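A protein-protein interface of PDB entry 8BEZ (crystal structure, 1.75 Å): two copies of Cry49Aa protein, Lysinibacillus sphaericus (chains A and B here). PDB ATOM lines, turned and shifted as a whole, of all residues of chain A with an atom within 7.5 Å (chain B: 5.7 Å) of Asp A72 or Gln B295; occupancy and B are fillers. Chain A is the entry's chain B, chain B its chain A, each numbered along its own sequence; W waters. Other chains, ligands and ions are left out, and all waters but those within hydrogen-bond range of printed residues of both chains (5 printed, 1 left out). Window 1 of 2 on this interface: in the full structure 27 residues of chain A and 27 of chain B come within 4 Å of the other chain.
The side-chain carboxylate of Asp B299 sits close to the side-chain carboxylate of Asp A299. The guanidinium group (NH2) of Arg B294 lies close to the side-chain amide nitrogen (ND2) of Asn A74 (3.2 Å). The backbone carbonyl oxygen (O) of Asp B72 lies within hydrogen-bond range of the side-chain amide nitrogen (NE2) of Gln A295 (3.4 Å). The side-chain amide nitrogen (ND2) of Asn A3 lies within hydrogen-bond range of the backbone carbonyl oxygen (O) of Ile B298 (3.0 Å). O of Asp A72 lies within hydrogen-bond range of NE2 of Gln B295 (3.4 Å).
OD2 of Asp B72 is in hydrogen-bond range of N of Arg B294, at 3.2 Å. The side-chain amide nitrogen (NE2) of Gln A296 lies within hydrogen-bond range of the side-chain carboxylate (OD1) of Asp A72, 2.9 Å away. OD1 of Asp A299 sits close to OE1 of Gln A295, at 2.8 Å. The side-chain carboxylate of Asp A72 lies within hydrogen-bond range of the backbone NH of Arg A294, at 3.2 Å. The side-chain carboxylate (OD1) of Asp B299 lies close to the side-chain amide oxygen (OE1) of Gln B295 (2.8 Å). The side-chain amide nitrogen (ND2) of Asn B300 is in hydrogen-bond range of the backbone carbonyl oxygen (O) of Gln B296.
Among the printed residues, pairs that only touch across the chains: Gln A295 with Gln B296 (3.5 Å), Gln A296 with Gln B295 (3.6 Å), Asn A3 with Asp B299 (3.8 Å), Asp A299 with Gln B296 (3.9 Å) and Gln A296 with Asp B299 (3.9 Å).
Asp A72 touches one residue of chain B. Pro A292 touches none of the printed residues of chain B. Printed residues of chain B within 4 Å of Gln A295: Asp B72 and Gln B296. Of the printed residues of chain A, Asp B72 touches Gln A295 (3.4 Å). Printed residues of chain A within 4 Å of Arg B294: Asn A74. Of chain A, only Asp A72 (3.4 Å) and Gln A296 (3.6 Å) come within 4 Å of Gln B295. Printed residues of chain A within 4 Å of Asp B299: Asn A3, Gln A296 and Asp A299. The nearest residue of chain A that does not touch Gln B295 is Asp A299 (4.02 Å). The nearest printed residue of chain A that does not touch Gln B296 is Asp A72 (6.8 Å).
Of the 20 printed residues of chain A, 6 touch a printed residue of chain B. Printed residues of chain B that touch a printed residue of chain A: Asp B72, Arg B294, Gln B295, Gln B296, Ile B298 and Asp B299. Among the printed residues, no Asp or Glu carboxylate lies within 4 Å of a Lys or Arg side-chain nitrogen of the other chain.
Asp A72 touches Gln B295, and with the chains exchanged Gln A295 touches Asp B72. Gln A295 touches Gln B296, and with the chains exchanged Gln A296 touches Gln B295. Gln A296 touches Asp B299, and with the chains exchanged Asp A299 touches Gln B296. Asp B299 touches its own counterpart, Asp A299. Of the 10 pairs that touch across the chains among the printed residues, 7 have their exchanged pair printed and touching as well.
Water W5 lies within hydrogen-bond range of O of Asp B299 (2.5 Å) and ND2 of Asn A3 (3.0 Å). Water W4 lies within hydrogen-bond range of the guanidinium group (NH2) of Arg B294 and the side-chain amide nitrogen (ND2) of Asn A74. Water W3 lies within hydrogen-bond range of NE2 of Gln B295, O of Asp A72 and NE of Arg B294. Water W2 bridges OD2 of Asp B72 and O of Asp A72. Water W1 bridges OD2 of Asp A72 and O of Asp B72.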
ATOM      1  N   ASN A   3     -21.755  23.127  12.037  1.00  0.00           N
ATOM      2  CA  ASN A   3     -21.971  24.594  11.963  1.00  0.00           C
ATOM      3  C   ASN A   3     -23.471  24.916  11.953  1.00  0.00           C
ATOM      4  O   ASN A   3     -23.917  25.589  11.009  1.00  0.00           O
ATOM      5  CB  ASN A   3     -21.265  25.132  10.720  1.00  0.00           C
ATOM      6  CG  ASN A   3     -20.619  26.479  10.945  1.00  0.00           C
ATOM      7  OD1 ASN A   3     -20.171  26.794  12.053  1.00  0.00           O
ATOM      8  ND2 ASN A   3     -20.548  27.266   9.886  1.00  0.00           N
ATOM      9  N   LEU A   4     -24.229  24.453  12.951  1.00  0.00           N
ATOM     10  CA  LEU A   4     -25.698  24.669  13.008  1.00  0.00           C
ATOM     11  C   LEU A   4     -26.057  25.472  14.247  1.00  0.00           C
ATOM     12  O   LEU A   4     -25.436  25.330  15.303  1.00  0.00           O
ATOM     13  CB  LEU A   4     -26.447  23.333  13.011  1.00  0.00           C
ATOM     14  CG  LEU A   4     -26.490  22.575  11.688  1.00  0.00           C
ATOM     15  CD1 LEU A   4     -27.102  21.202  11.901  1.00  0.00           C
ATOM     16  CD2 LEU A   4     -27.277  23.342  10.622  1.00  0.00           C
ATOM     17  N   TYR A  69     -35.363  23.619  11.469  1.00  0.00           N
ATOM     18  CA  TYR A  69     -34.468  23.263  10.343  1.00  0.00           C
ATOM     19  C   TYR A  69     -33.998  24.558   9.681  1.00  0.00           C
ATOM     20  O   TYR A  69     -34.860  25.384   9.222  1.00  0.00           O
ATOM     21  CB  TYR A  69     -35.154  22.309   9.369  1.00  0.00           C
ATOM     22  CG  TYR A  69     -35.370  20.914   9.888  1.00  0.00           C
ATOM     23  CD1 TYR A  69     -34.311  20.048  10.142  1.00  0.00           C
ATOM     24  CD2 TYR A  69     -36.661  20.430  10.068  1.00  0.00           C
ATOM     25  CE1 TYR A  69     -34.543  18.742  10.586  1.00  0.00           C
ATOM     26  CE2 TYR A  69     -36.902  19.129  10.479  1.00  0.00           C
ATOM     27  CZ  TYR A  69     -35.843  18.285  10.767  1.00  0.00           C
ATOM     28  OH  TYR A  69     -36.117  16.999  11.173  1.00  0.00           O
ATOM     29  N   ALA A  70     -32.669  24.732   9.604  1.00  0.00           N
ATOM     30  CA  ALA A  70     -32.006  25.964   9.122  1.00  0.00           C
ATOM     31  C   ALA A  70     -31.954  25.959   7.593  1.00  0.00           C
ATOM     32  O   ALA A  70     -31.280  25.041   6.979  1.00  0.00           O
ATOM     33  CB  ALA A  70     -30.627  26.111   9.727  1.00  0.00           C
ATOM     34  N   LEU A  71     -32.585  26.963   6.987  1.00  0.00           N
ATOM     35  CA  LEU A  71     -32.549  27.202   5.519  1.00  0.00           C
ATOM     36  C   LEU A  71     -31.292  28.004   5.176  1.00  0.00           C
ATOM     37  O   LEU A  71     -30.748  28.727   6.077  1.00  0.00           O
ATOM     38  CB  LEU A  71     -33.816  27.955   5.104  1.00  0.00           C
ATOM     39  CG  LEU A  71     -35.148  27.309   5.485  1.00  0.00           C
ATOM     40  CD1 LEU A  71     -36.310  28.180   5.034  1.00  0.00           C
ATOM     41  CD2 LEU A  71     -35.273  25.932   4.879  1.00  0.00           C
ATOM     42  N   ASP A  72     -30.844  27.925   3.915  1.00  0.00           N
ATOM     43  CA  ASP A  72     -29.703  28.720   3.410  1.00  0.00           C
ATOM     44  C   ASP A  72     -29.931  30.227   3.636  1.00  0.00           C
ATOM     45  O   ASP A  72     -28.906  30.994   3.691  1.00  0.00           O
ATOM     46  CB  ASP A  72     -29.483  28.471   1.910  1.00  0.00           C
ATOM     47  CG  ASP A  72     -29.027  27.080   1.510  1.00  0.00           C
ATOM     48  OD1 ASP A  72     -28.671  26.276   2.430  1.00  0.00           O
ATOM     49  OD2 ASP A  72     -28.995  26.818   0.251  1.00  0.00           O
ATOM     50  N   ASN A  73     -31.188  30.690   3.652  1.00  0.00           N
ATOM     51  CA  ASN A  73     -31.508  32.140   3.758  1.00  0.00           C
ATOM     52  C   ASN A  73     -31.650  32.582   5.223  1.00  0.00           C
ATOM     53  O   ASN A  73     -32.045  33.755   5.460  1.00  0.00           O
ATOM     54  CB  ASN A  73     -32.767  32.510   2.979  1.00  0.00           C
ATOM     55  CG  ASN A  73     -34.033  31.856   3.481  1.00  0.00           C
ATOM     56  OD1 ASN A  73     -34.096  31.239   4.567  1.00  0.00           O
ATOM     57  ND2 ASN A  73     -35.064  32.006   2.664  1.00  0.00           N
ATOM     58  N   ASN A  74     -31.312  31.719   6.172  1.00  0.00           N
ATOM     59  CA  ASN A  74     -31.225  32.092   7.616  1.00  0.00           C
ATOM     60  C   ASN A  74     -32.605  32.069   8.277  1.00  0.00           C
ATOM     61  O   ASN A  74     -32.688  32.383   9.520  1.00  0.00           O
ATOM     62  CB  ASN A  74     -30.602  33.473   7.862  1.00  0.00           C
ATOM     63  CG  ASN A  74     -29.945  33.531   9.225  1.00  0.00           C
ATOM     64  OD1 ASN A  74     -29.277  32.565   9.608  1.00  0.00           O
ATOM     65  ND2 ASN A  74     -30.138  34.620   9.963  1.00  0.00           N
ATOM     66  N   ASN A  75     -33.642  31.689   7.531  1.00  0.00           N
ATOM     67  CA  ASN A  75     -34.967  31.380   8.118  1.00  0.00           C
ATOM     68  C   ASN A  75     -35.023  29.901   8.497  1.00  0.00           C
ATOM     69  O   ASN A  75     -34.035  29.117   8.224  1.00  0.00           O
ATOM     70  CB  ASN A  75     -36.080  31.811   7.162  1.00  0.00           C
ATOM     71  CG  ASN A  75     -36.032  33.296   6.889  1.00  0.00           C
ATOM     72  OD1 ASN A  75     -35.740  34.097   7.774  1.00  0.00           O
ATOM     73  ND2 ASN A  75     -36.239  33.673   5.643  1.00  0.00           N
ATOM     74  N   SER A 290     -35.679  20.010  -1.837  1.00  0.00           N
ATOM     75  CA  SER A 290     -34.273  20.047  -1.348  1.00  0.00           C
ATOM     76  C   SER A 290     -33.653  21.428  -1.586  1.00  0.00           C
ATOM     77  O   SER A 290     -32.635  21.785  -0.854  1.00  0.00           O
ATOM     78  CB  SER A 290     -33.459  18.949  -2.001  1.00  0.00           C
ATOM     79  OG  SER A 290     -33.506  19.080  -3.430  1.00  0.00           O
ATOM     80  N   THR A 291     -34.203  22.201  -2.548  1.00  0.00           N
ATOM     81  CA  THR A 291     -33.656  23.517  -2.993  1.00  0.00           C
ATOM     82  C   THR A 291     -33.353  24.468  -1.832  1.00  0.00           C
ATOM     83  O   THR A 291     -32.351  25.203  -1.892  1.00  0.00           O
ATOM     84  CB  THR A 291     -34.565  24.168  -4.052  1.00  0.00           C
ATOM     85  OG1 THR A 291     -34.264  23.523  -5.293  1.00  0.00           O
ATOM     86  CG2 THR A 291     -34.344  25.652  -4.229  1.00  0.00           C
ATOM     87  N   PRO A 292     -34.218  24.590  -0.787  1.00  0.00           N
ATOM     88  CA  PRO A 292     -33.990  25.567   0.286  1.00  0.00           C
ATOM     89  C   PRO A 292     -32.728  25.321   1.143  1.00  0.00           C
ATOM     90  O   PRO A 292     -32.282  26.266   1.890  1.00  0.00           O
ATOM     91  CB  PRO A 292     -35.247  25.441   1.161  1.00  0.00           C
ATOM     92  CG  PRO A 292     -36.289  24.836   0.243  1.00  0.00           C
ATOM     93  CD  PRO A 292     -35.507  23.898  -0.648  1.00  0.00           C
ATOM     94  N   PHE A 293     -32.166  24.108   1.035  1.00  0.00           N
ATOM     95  CA  PHE A 293     -30.950  23.633   1.750  1.00  0.00           C
ATOM     96  C   PHE A 293     -29.752  23.410   0.818  1.00  0.00           C
ATOM     97  O   PHE A 293     -28.698  22.872   1.305  1.00  0.00           O
ATOM     98  CB  PHE A 293     -31.256  22.299   2.441  1.00  0.00           C
ATOM     99  CG  PHE A 293     -32.434  22.365   3.378  1.00  0.00           C
ATOM    100  CD1 PHE A 293     -32.273  22.821   4.671  1.00  0.00           C
ATOM    101  CD2 PHE A 293     -33.701  22.017   2.947  1.00  0.00           C
ATOM    102  CE1 PHE A 293     -33.367  22.923   5.530  1.00  0.00           C
ATOM    103  CE2 PHE A 293     -34.790  22.103   3.805  1.00  0.00           C
ATOM    104  CZ  PHE A 293     -34.620  22.541   5.097  1.00  0.00           C
ATOM    105  N   ARG A 294     -29.858  23.790  -0.463  1.00  0.00           N
ATOM    106  CA  ARG A 294     -28.895  23.328  -1.505  1.00  0.00           C
ATOM    107  C   ARG A 294     -27.453  23.754  -1.183  1.00  0.00           C
ATOM    108  O   ARG A 294     -26.529  22.911  -1.420  1.00  0.00           O
ATOM    109  CB  ARG A 294     -29.316  23.782  -2.910  1.00  0.00           C
ATOM    110  CG  ARG A 294     -29.419  25.283  -3.133  1.00  0.00           C
ATOM    111  CD  ARG A 294     -29.760  25.552  -4.593  1.00  0.00           C
ATOM    112  NE  ARG A 294     -28.654  25.086  -5.411  1.00  0.00           N
ATOM    113  CZ  ARG A 294     -28.754  24.615  -6.642  1.00  0.00           C
ATOM    114  NH1 ARG A 294     -27.673  24.197  -7.261  1.00  0.00           N
ATOM    115  NH2 ARG A 294     -29.920  24.542  -7.246  1.00  0.00           N
ATOM    116  N   GLN A 295     -27.214  24.988  -0.710  1.00  0.00           N
ATOM    117  CA  GLN A 295     -25.828  25.482  -0.498  1.00  0.00           C
ATOM    118  C   GLN A 295     -25.171  24.724   0.671  1.00  0.00           C
ATOM    119  O   GLN A 295     -23.965  24.366   0.564  1.00  0.00           O
ATOM    120  CB  GLN A 295     -25.780  26.997  -0.321  1.00  0.00           C
ATOM    121  CG  GLN A 295     -24.361  27.550  -0.324  1.00  0.00           C
ATOM    122  CD  GLN A 295     -23.640  27.327  -1.634  1.00  0.00           C
ATOM    123  OE1 GLN A 295     -22.509  26.827  -1.671  1.00  0.00           O
ATOM    124  NE2 GLN A 295     -24.285  27.710  -2.730  1.00  0.00           N
ATOM    125  N   GLN A 296     -25.914  24.451   1.756  1.00  0.00           N
ATOM    126  CA  GLN A 296     -25.409  23.622   2.890  1.00  0.00           C
ATOM    127  C   GLN A 296     -25.070  22.214   2.380  1.00  0.00           C
ATOM    128  O   GLN A 296     -23.989  21.671   2.781  1.00  0.00           O
ATOM    129  CB  GLN A 296     -26.443  23.550   4.016  1.00  0.00           C
ATOM    130  CG  GLN A 296     -26.590  24.868   4.738  1.00  0.00           C
ATOM    131  CD  GLN A 296     -27.757  24.829   5.682  1.00  0.00           C
ATOM    132  OE1 GLN A 296     -27.638  24.371   6.843  1.00  0.00           O
ATOM    133  NE2 GLN A 296     -28.898  25.301   5.185  1.00  0.00           N
ATOM    134  N   ILE A 297     -25.938  21.625   1.560  1.00  0.00           N
ATOM    135  CA  ILE A 297     -25.761  20.234   1.039  1.00  0.00           C
ATOM    136  C   ILE A 297     -24.480  20.198   0.187  1.00  0.00           C
ATOM    137  O   ILE A 297     -23.606  19.296   0.425  1.00  0.00           O
ATOM    138  CB  ILE A 297     -27.025  19.738   0.309  1.00  0.00           C
ATOM    139  CG1 ILE A 297     -28.165  19.517   1.313  1.00  0.00           C
ATOM    140  CG2 ILE A 297     -26.749  18.486  -0.520  1.00  0.00           C
ATOM    141  CD1 ILE A 297     -29.509  19.283   0.691  1.00  0.00           C
ATOM    142  N   ILE A 298     -24.324  21.159  -0.739  1.00  0.00           N
ATOM    143  CA  ILE A 298     -23.128  21.290  -1.625  1.00  0.00           C
ATOM    144  C   ILE A 298     -21.856  21.466  -0.798  1.00  0.00           C
ATOM    145  O   ILE A 298     -20.856  20.710  -1.057  1.00  0.00           O
ATOM    146  CB  ILE A 298     -23.374  22.453  -2.614  1.00  0.00           C
ATOM    147  CG1 ILE A 298     -24.293  21.979  -3.744  1.00  0.00           C
ATOM    148  CG2 ILE A 298     -22.098  23.064  -3.137  1.00  0.00           C
ATOM    149  CD1 ILE A 298     -24.998  23.132  -4.446  1.00  0.00           C
ATOM    150  N   ASP A 299     -21.867  22.427   0.134  1.00  0.00           N
ATOM    151  CA  ASP A 299     -20.681  22.819   0.946  1.00  0.00           C
ATOM    152  C   ASP A 299     -20.245  21.572   1.749  1.00  0.00           C
ATOM    153  O   ASP A 299     -19.041  21.249   1.755  1.00  0.00           O
ATOM    154  CB  ASP A 299     -20.966  24.055   1.820  1.00  0.00           C
ATOM    155  CG  ASP A 299     -21.031  25.432   1.132  1.00  0.00           C
ATOM    156  OD1 ASP A 299     -20.582  25.531  -0.050  1.00  0.00           O
ATOM    157  OD2 ASP A 299     -21.497  26.435   1.798  1.00  0.00           O
ATOM    158  N   ASN A 300     -21.173  20.870   2.409  1.00  0.00           N
ATOM    159  CA  ASN A 300     -20.834  19.782   3.366  1.00  0.00           C
ATOM    160  C   ASN A 300     -20.539  18.477   2.623  1.00  0.00           C
ATOM    161  O   ASN A 300     -19.600  17.744   3.066  1.00  0.00           O
ATOM    162  CB  ASN A 300     -21.927  19.611   4.423  1.00  0.00           C
ATOM    163  CG  ASN A 300     -22.030  20.817   5.325  1.00  0.00           C
ATOM    164  OD1 ASN A 300     -23.111  21.359   5.482  1.00  0.00           O
ATOM    165  ND2 ASN A 300     -20.940  21.237   5.927  1.00  0.00           N
ATOM    166  N   ASP B  72     -25.331  32.001  -3.336  1.00  0.00           N
ATOM    167  CA  ASP B  72     -25.921  30.859  -2.596  1.00  0.00           C
ATOM    168  C   ASP B  72     -27.065  30.188  -3.399  1.00  0.00           C
ATOM    169  O   ASP B  72     -27.368  28.973  -3.147  1.00  0.00           O
ATOM    170  CB  ASP B  72     -26.456  31.305  -1.229  1.00  0.00           C
ATOM    171  CG  ASP B  72     -25.428  31.785  -0.213  1.00  0.00           C
ATOM    172  OD1 ASP B  72     -24.179  31.618  -0.465  1.00  0.00           O
ATOM    173  OD2 ASP B  72     -25.875  32.314   0.854  1.00  0.00           O
ATOM    174  N   THR B 291     -25.310  39.736   1.713  1.00  0.00           N
ATOM    175  CA  THR B 291     -26.432  38.767   1.922  1.00  0.00           C
ATOM    176  C   THR B 291     -26.455  37.640   0.884  1.00  0.00           C
ATOM    177  O   THR B 291     -26.760  36.486   1.246  1.00  0.00           O
ATOM    178  CB  THR B 291     -27.785  39.489   2.015  1.00  0.00           C
ATOM    179  OG1 THR B 291     -27.863  40.015   3.344  1.00  0.00           O
ATOM    180  CG2 THR B 291     -28.982  38.598   1.789  1.00  0.00           C
ATOM    181  N   PHE B 293     -24.267  35.953  -0.562  1.00  0.00           N
ATOM    182  CA  PHE B 293     -23.137  35.017  -0.307  1.00  0.00           C
ATOM    183  C   PHE B 293     -23.111  34.508   1.143  1.00  0.00           C
ATOM    184  O   PHE B 293     -22.106  33.790   1.512  1.00  0.00           O
ATOM    185  CB  PHE B 293     -21.809  35.727  -0.574  1.00  0.00           C
ATOM    186  CG  PHE B 293     -21.696  36.311  -1.956  1.00  0.00           C
ATOM    187  CD1 PHE B 293     -21.300  35.520  -3.015  1.00  0.00           C
ATOM    188  CD2 PHE B 293     -22.033  37.641  -2.193  1.00  0.00           C
ATOM    189  CE1 PHE B 293     -21.223  36.049  -4.300  1.00  0.00           C
ATOM    190  CE2 PHE B 293     -21.940  38.174  -3.479  1.00  0.00           C
ATOM    191  CZ  PHE B 293     -21.517  37.385  -4.526  1.00  0.00           C
ATOM    192  N   ARG B 294     -24.146  34.812   1.948  1.00  0.00           N
ATOM    193  CA  ARG B 294     -24.089  34.626   3.425  1.00  0.00           C
ATOM    194  C   ARG B 294     -23.791  33.167   3.802  1.00  0.00           C
ATOM    195  O   ARG B 294     -22.983  32.982   4.783  1.00  0.00           O
ATOM    196  CB  ARG B 294     -25.347  35.152   4.130  1.00  0.00           C
ATOM    197  CG  ARG B 294     -26.655  34.469   3.747  1.00  0.00           C
ATOM    198  CD  ARG B 294     -27.852  34.976   4.545  1.00  0.00           C
ATOM    199  NE  ARG B 294     -27.622  34.660   5.943  1.00  0.00           N
ATOM    200  CZ  ARG B 294     -27.847  35.463   6.988  1.00  0.00           C
ATOM    201  NH1 ARG B 294     -28.384  36.672   6.837  1.00  0.00           N
ATOM    202  NH2 ARG B 294     -27.531  35.031   8.200  1.00  0.00           N
ATOM    203  N   GLN B 295     -24.436  32.169   3.170  1.00  0.00           N
ATOM    204  CA  GLN B 295     -24.295  30.753   3.601  1.00  0.00           C
ATOM    205  C   GLN B 295     -22.862  30.264   3.336  1.00  0.00           C
ATOM    206  O   GLN B 295     -22.281  29.548   4.221  1.00  0.00           O
ATOM    207  CB  GLN B 295     -25.357  29.839   2.995  1.00  0.00           C
ATOM    208  CG  GLN B 295     -25.377  28.453   3.637  1.00  0.00           C
ATOM    209  CD  GLN B 295     -25.674  28.479   5.122  1.00  0.00           C
ATOM    210  OE1 GLN B 295     -24.976  27.849   5.922  1.00  0.00           O
ATOM    211  NE2 GLN B 295     -26.704  29.223   5.516  1.00  0.00           N
ATOM    212  N   GLN B 296     -22.283  30.617   2.183  1.00  0.00           N
ATOM    213  CA  GLN B 296     -20.859  30.290   1.865  1.00  0.00           C
ATOM    214  C   GLN B 296     -19.928  30.943   2.895  1.00  0.00           C
ATOM    215  O   GLN B 296     -18.954  30.255   3.367  1.00  0.00           O
ATOM    216  CB  GLN B 296     -20.516  30.755   0.450  1.00  0.00           C
ATOM    217  CG  GLN B 296     -21.221  29.941  -0.611  1.00  0.00           C
ATOM    218  CD  GLN B 296     -21.041  30.569  -1.969  1.00  0.00           C
ATOM    219  OE1 GLN B 296     -20.030  30.340  -2.641  1.00  0.00           O
ATOM    220  NE2 GLN B 296     -22.023  31.370  -2.376  1.00  0.00           N
ATOM    221  N   ILE B 297     -20.180  32.206   3.247  1.00  0.00           N
ATOM    222  CA  ILE B 297     -19.326  32.967   4.203  1.00  0.00           C
ATOM    223  C   ILE B 297     -19.380  32.268   5.575  1.00  0.00           C
ATOM    224  O   ILE B 297     -18.277  31.975   6.173  1.00  0.00           O
ATOM    225  CB  ILE B 297     -19.696  34.468   4.221  1.00  0.00           C
ATOM    226  CG1 ILE B 297     -19.309  35.128   2.890  1.00  0.00           C
ATOM    227  CG2 ILE B 297     -19.079  35.176   5.418  1.00  0.00           C
ATOM    228  CD1 ILE B 297     -19.852  36.528   2.700  1.00  0.00           C
ATOM    229  N   ILE B 298     -20.587  31.938   6.054  1.00  0.00           N
ATOM    230  CA  ILE B 298     -20.816  31.236   7.355  1.00  0.00           C
ATOM    231  C   ILE B 298     -20.124  29.870   7.363  1.00  0.00           C
ATOM    232  O   ILE B 298     -19.373  29.561   8.362  1.00  0.00           O
ATOM    233  CB  ILE B 298     -22.341  31.137   7.594  1.00  0.00           C
ATOM    234  CG1 ILE B 298     -22.874  32.482   8.090  1.00  0.00           C
ATOM    235  CG2 ILE B 298     -22.715  30.004   8.518  1.00  0.00           C
ATOM    236  CD1 ILE B 298     -24.360  32.638   7.838  1.00  0.00           C
ATOM    237  N   ASP B 299     -20.368  29.068   6.316  1.00  0.00           N
ATOM    238  CA  ASP B 299     -19.892  27.667   6.207  1.00  0.00           C
ATOM    239  C   ASP B 299     -18.357  27.703   6.254  1.00  0.00           C
ATOM    240  O   ASP B 299     -17.766  26.928   7.048  1.00  0.00           O
ATOM    241  CB  ASP B 299     -20.472  26.949   4.969  1.00  0.00           C
ATOM    242  CG  ASP B 299     -21.933  26.477   5.043  1.00  0.00           C
ATOM    243  OD1 ASP B 299     -22.496  26.506   6.178  1.00  0.00           O
ATOM    244  OD2 ASP B 299     -22.521  26.060   3.960  1.00  0.00           O
ATOM    245  N   ASN B 300     -17.718  28.569   5.457  1.00  0.00           N
ATOM    246  CA  ASN B 300     -16.241  28.556   5.283  1.00  0.00           C
ATOM    247  C   ASN B 300     -15.531  29.240   6.452  1.00  0.00           C
ATOM    248  O   ASN B 300     -14.428  28.723   6.848  1.00  0.00           O
ATOM    249  CB  ASN B 300     -15.852  29.119   3.915  1.00  0.00           C
ATOM    250  CG  ASN B 300     -16.262  28.155   2.826  1.00  0.00           C
ATOM    251  OD1 ASN B 300     -15.804  27.012   2.780  1.00  0.00           O
ATOM    252  ND2 ASN B 300     -17.174  28.559   1.982  1.00  0.00           N
HETATM  253  O   HOH W   1     -29.548  28.766  -1.512  1.00  0.00           O
HETATM  254  O   HOH W   2     -28.499  32.356   1.288  1.00  0.00           O
HETATM  255  O   HOH W   3     -27.426  31.721   6.047  1.00  0.00           O
HETATM  256  O   HOH W   4     -27.500  36.861  10.073  1.00  0.00           O
HETATM  257  O   HOH W   5     -18.734  25.241   8.677  1.00  0.00           O
